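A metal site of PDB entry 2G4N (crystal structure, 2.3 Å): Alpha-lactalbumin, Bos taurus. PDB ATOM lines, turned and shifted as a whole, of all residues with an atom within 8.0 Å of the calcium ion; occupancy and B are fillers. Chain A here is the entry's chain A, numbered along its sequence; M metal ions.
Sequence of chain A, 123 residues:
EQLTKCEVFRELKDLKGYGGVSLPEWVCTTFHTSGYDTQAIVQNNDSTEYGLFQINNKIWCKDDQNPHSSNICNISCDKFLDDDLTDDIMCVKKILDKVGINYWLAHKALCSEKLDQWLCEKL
OD1 of Asp 84 is in hydrogen-bond range of OG1 of Thr 86.
Of the 17 residues printed, 5 come within 4 Å of the calcium ion. The nearest printed residue that does not touch the calcium ion is Phe 80 (4.1 Å).
The calcium ion is bound by the side-chain carboxylate of Asp 88, the backbone carbonyl oxygen of Asp 84, the backbone carbonyl oxygen of Lys 79, the side-chain carboxylate of Asp 82 and the side-chain carboxylate of Asp 87.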
ATOM      1  N   THR A  38      -8.309 -32.140  16.023  1.00  0.00           N
ATOM      2  CA  THR A  38      -8.362 -30.690  15.896  1.00  0.00           C
ATOM      3  C   THR A  38      -9.251 -30.025  16.958  1.00  0.00           C
ATOM      4  O   THR A  38      -9.226 -28.864  17.048  1.00  0.00           O
ATOM      5  CB  THR A  38      -8.893 -30.222  14.483  1.00  0.00           C
ATOM      6  OG1 THR A  38     -10.244 -30.674  14.257  1.00  0.00           O
ATOM      7  CG2 THR A  38      -7.987 -30.658  13.349  1.00  0.00           C
ATOM      8  N   ILE A  55      -2.739 -24.893  21.872  1.00  0.00           N
ATOM      9  CA  ILE A  55      -2.352 -23.485  22.035  1.00  0.00           C
ATOM     10  C   ILE A  55      -3.098 -22.997  23.218  1.00  0.00           C
ATOM     11  O   ILE A  55      -4.293 -23.140  23.246  1.00  0.00           O
ATOM     12  CB  ILE A  55      -2.746 -22.576  20.797  1.00  0.00           C
ATOM     13  CG1 ILE A  55      -1.936 -23.025  19.631  1.00  0.00           C
ATOM     14  CG2 ILE A  55      -2.402 -21.032  21.007  1.00  0.00           C
ATOM     15  CD1 ILE A  55      -2.506 -22.588  18.299  1.00  0.00           C
ATOM     16  N   ILE A  75      -6.484 -13.315  18.782  1.00  0.00           N
ATOM     17  CA  ILE A  75      -7.500 -14.235  18.316  1.00  0.00           C
ATOM     18  C   ILE A  75      -8.215 -14.952  19.429  1.00  0.00           C
ATOM     19  O   ILE A  75      -7.649 -15.230  20.479  1.00  0.00           O
ATOM     20  CB  ILE A  75      -6.796 -15.302  17.339  1.00  0.00           C
ATOM     21  CG1 ILE A  75      -7.810 -15.896  16.371  1.00  0.00           C
ATOM     22  CG2 ILE A  75      -6.026 -16.360  18.101  1.00  0.00           C
ATOM     23  CD1 ILE A  75      -7.248 -16.947  15.436  1.00  0.00           C
ATOM     24  N   SER A  76      -9.496 -15.257  19.232  1.00  0.00           N
ATOM     25  CA  SER A  76     -10.212 -16.317  20.013  1.00  0.00           C
ATOM     26  C   SER A  76      -9.665 -17.714  19.840  1.00  0.00           C
ATOM     27  O   SER A  76      -9.565 -18.225  18.761  1.00  0.00           O
ATOM     28  CB  SER A  76     -11.693 -16.398  19.613  1.00  0.00           C
ATOM     29  OG  SER A  76     -12.239 -15.107  19.741  1.00  0.00           O
ATOM     30  N   CYS A  77      -9.379 -18.326  20.973  1.00  0.00           N
ATOM     31  CA  CYS A  77      -8.931 -19.686  21.090  1.00  0.00           C
ATOM     32  C   CYS A  77      -9.773 -20.660  20.371  1.00  0.00           C
ATOM     33  O   CYS A  77      -9.282 -21.611  19.798  1.00  0.00           O
ATOM     34  CB  CYS A  77      -9.019 -20.064  22.558  1.00  0.00           C
ATOM     35  SG  CYS A  77      -7.803 -19.250  23.605  1.00  0.00           S
ATOM     36  N   ASP A  78     -11.061 -20.463  20.400  1.00  0.00           N
ATOM     37  CA  ASP A  78     -11.899 -21.371  19.691  1.00  0.00           C
ATOM     38  C   ASP A  78     -11.817 -21.362  18.097  1.00  0.00           C
ATOM     39  O   ASP A  78     -12.146 -22.358  17.469  1.00  0.00           O
ATOM     40  CB  ASP A  78     -13.266 -21.378  20.335  1.00  0.00           C
ATOM     41  CG  ASP A  78     -13.983 -20.208  20.103  1.00  0.00           C
ATOM     42  OD1 ASP A  78     -14.850 -19.908  21.009  1.00  0.00           O
ATOM     43  OD2 ASP A  78     -13.656 -19.615  19.024  1.00  0.00           O
ATOM     44  N   LYS A  79     -11.208 -20.337  17.499  1.00  0.00           N
ATOM     45  CA  LYS A  79     -10.731 -20.461  16.144  1.00  0.00           C
ATOM     46  C   LYS A  79      -9.721 -21.622  15.989  1.00  0.00           C
ATOM     47  O   LYS A  79      -9.367 -22.012  14.890  1.00  0.00           O
ATOM     48  CB  LYS A  79     -10.147 -19.119  15.641  1.00  0.00           C
ATOM     49  CG  LYS A  79     -11.196 -18.025  15.346  1.00  0.00           C
ATOM     50  CD  LYS A  79     -12.098 -18.501  14.153  1.00  0.00           C
ATOM     51  CE  LYS A  79     -13.063 -17.478  13.629  1.00  0.00           C
ATOM     52  NZ  LYS A  79     -13.255 -17.614  12.121  1.00  0.00           N
ATOM     53  N   PHE A  80      -9.221 -22.170  17.091  1.00  0.00           N
ATOM     54  CA  PHE A  80      -8.224 -23.257  17.017  1.00  0.00           C
ATOM     55  C   PHE A  80      -8.879 -24.638  17.139  1.00  0.00           C
ATOM     56  O   PHE A  80      -8.216 -25.621  17.230  1.00  0.00           O
ATOM     57  CB  PHE A  80      -7.139 -23.091  18.078  1.00  0.00           C
ATOM     58  CG  PHE A  80      -6.251 -21.810  17.931  1.00  0.00           C
ATOM     59  CD1 PHE A  80      -5.780 -21.159  19.081  1.00  0.00           C
ATOM     60  CD2 PHE A  80      -5.912 -21.275  16.683  1.00  0.00           C
ATOM     61  CE1 PHE A  80      -4.977 -20.012  18.989  1.00  0.00           C
ATOM     62  CE2 PHE A  80      -5.110 -20.109  16.585  1.00  0.00           C
ATOM     63  CZ  PHE A  80      -4.582 -19.507  17.735  1.00  0.00           C
ATOM     64  N   LEU A  81     -10.211 -24.701  17.028  1.00  0.00           N
ATOM     65  CA  LEU A  81     -10.922 -25.971  17.147  1.00  0.00           C
ATOM     66  C   LEU A  81     -11.650 -26.356  15.880  1.00  0.00           C
ATOM     67  O   LEU A  81     -12.328 -27.395  15.853  1.00  0.00           O
ATOM     68  CB  LEU A  81     -11.916 -25.851  18.285  1.00  0.00           C
ATOM     69  CG  LEU A  81     -11.301 -25.507  19.685  1.00  0.00           C
ATOM     70  CD1 LEU A  81     -12.496 -25.095  20.638  1.00  0.00           C
ATOM     71  CD2 LEU A  81     -10.547 -26.657  20.198  1.00  0.00           C
ATOM     72  N   ASP A  82     -11.593 -25.515  14.838  1.00  0.00           N
ATOM     73  CA  ASP A  82     -12.160 -25.882  13.568  1.00  0.00           C
ATOM     74  C   ASP A  82     -11.092 -26.631  12.696  1.00  0.00           C
ATOM     75  O   ASP A  82     -10.051 -27.095  13.232  1.00  0.00           O
ATOM     76  CB  ASP A  82     -12.819 -24.705  12.915  1.00  0.00           C
ATOM     77  CG  ASP A  82     -11.835 -23.597  12.512  1.00  0.00           C
ATOM     78  OD1 ASP A  82     -10.580 -23.804  12.633  1.00  0.00           O
ATOM     79  OD2 ASP A  82     -12.389 -22.505  12.124  1.00  0.00           O
ATOM     80  N   ASP A  83     -11.408 -26.875  11.452  1.00  0.00           N
ATOM     81  CA  ASP A  83     -10.632 -27.736  10.563  1.00  0.00           C
ATOM     82  C   ASP A  83      -9.604 -26.949   9.717  1.00  0.00           C
ATOM     83  O   ASP A  83      -8.665 -27.536   9.144  1.00  0.00           O
ATOM     84  CB  ASP A  83     -11.573 -28.431   9.521  1.00  0.00           C
ATOM     85  CG  ASP A  83     -12.599 -29.417  10.143  1.00  0.00           C
ATOM     86  OD1 ASP A  83     -12.472 -29.913  11.270  1.00  0.00           O
ATOM     87  OD2 ASP A  83     -13.570 -29.713   9.449  1.00  0.00           O
ATOM     88  N   ASP A  84      -9.872 -25.657   9.512  1.00  0.00           N
ATOM     89  CA  ASP A  84      -8.976 -24.750   8.819  1.00  0.00           C
ATOM     90  C   ASP A  84      -7.908 -24.413   9.826  1.00  0.00           C
ATOM     91  O   ASP A  84      -8.148 -23.744  10.826  1.00  0.00           O
ATOM     92  CB  ASP A  84      -9.678 -23.482   8.380  1.00  0.00           C
ATOM     93  CG  ASP A  84      -8.857 -22.673   7.355  1.00  0.00           C
ATOM     94  OD1 ASP A  84      -7.655 -22.961   7.201  1.00  0.00           O
ATOM     95  OD2 ASP A  84      -9.437 -21.748   6.717  1.00  0.00           O
ATOM     96  N   LEU A  85      -6.717 -24.929   9.568  1.00  0.00           N
ATOM     97  CA  LEU A  85      -5.589 -24.743  10.398  1.00  0.00           C
ATOM     98  C   LEU A  85      -4.785 -23.543   9.909  1.00  0.00           C
ATOM     99  O   LEU A  85      -3.708 -23.340  10.405  1.00  0.00           O
ATOM    100  CB  LEU A  85      -4.708 -25.997  10.343  1.00  0.00           C
ATOM    101  CG  LEU A  85      -5.302 -27.363  10.726  1.00  0.00           C
ATOM    102  CD1 LEU A  85      -4.356 -28.540  10.380  1.00  0.00           C
ATOM    103  CD2 LEU A  85      -5.581 -27.286  12.142  1.00  0.00           C
ATOM    104  N   THR A  86      -5.280 -22.759   8.941  1.00  0.00           N
ATOM    105  CA  THR A  86      -4.548 -21.520   8.566  1.00  0.00           C
ATOM    106  C   THR A  86      -4.266 -20.624   9.839  1.00  0.00           C
ATOM    107  O   THR A  86      -3.112 -20.304  10.112  1.00  0.00           O
ATOM    108  CB  THR A  86      -5.244 -20.661   7.492  1.00  0.00           C
ATOM    109  OG1 THR A  86      -5.701 -21.449   6.409  1.00  0.00           O
ATOM    110  CG2 THR A  86      -4.259 -19.507   6.922  1.00  0.00           C
ATOM    111  N   ASP A  87      -5.269 -20.287  10.640  1.00  0.00           N
ATOM    112  CA  ASP A  87      -4.949 -19.325  11.739  1.00  0.00           C
ATOM    113  C   ASP A  87      -4.077 -20.053  12.802  1.00  0.00           C
ATOM    114  O   ASP A  87      -3.168 -19.443  13.367  1.00  0.00           O
ATOM    115  CB  ASP A  87      -6.185 -18.600  12.335  1.00  0.00           C
ATOM    116  CG  ASP A  87      -7.367 -19.581  12.670  1.00  0.00           C
ATOM    117  OD1 ASP A  87      -7.029 -20.778  12.798  1.00  0.00           O
ATOM    118  OD2 ASP A  87      -8.577 -19.169  12.751  1.00  0.00           O
ATOM    119  N   ASP A  88      -4.325 -21.356  13.020  1.00  0.00           N
ATOM    120  CA  ASP A  88      -3.547 -22.138  13.981  1.00  0.00           C
ATOM    121  C   ASP A  88      -2.047 -22.018  13.641  1.00  0.00           C
ATOM    122  O   ASP A  88      -1.208 -21.763  14.505  1.00  0.00           O
ATOM    123  CB  ASP A  88      -3.958 -23.629  13.932  1.00  0.00           C
ATOM    124  CG  ASP A  88      -5.422 -23.861  14.311  1.00  0.00           C
ATOM    125  OD1 ASP A  88      -6.277 -23.168  13.710  1.00  0.00           O
ATOM    126  OD2 ASP A  88      -5.700 -24.712  15.210  1.00  0.00           O
ATOM    127  N   ILE A  89      -1.725 -22.177  12.368  1.00  0.00           N
ATOM    128  CA  ILE A  89      -0.308 -22.115  11.908  1.00  0.00           C
ATOM    129  C   ILE A  89       0.359 -20.743  12.083  1.00  0.00           C
ATOM    130  O   ILE A  89       1.533 -20.646  12.484  1.00  0.00           O
ATOM    131  CB  ILE A  89      -0.152 -22.602  10.426  1.00  0.00           C
ATOM    132  CG1 ILE A  89      -0.457 -24.103  10.360  1.00  0.00           C
ATOM    133  CG2 ILE A  89       1.189 -22.246   9.952  1.00  0.00           C
ATOM    134  CD1 ILE A  89      -0.171 -24.838   9.008  1.00  0.00           C
HETATM  135 CA    CA M   1      -8.361 -22.878  12.919  1.00  0.00          CA
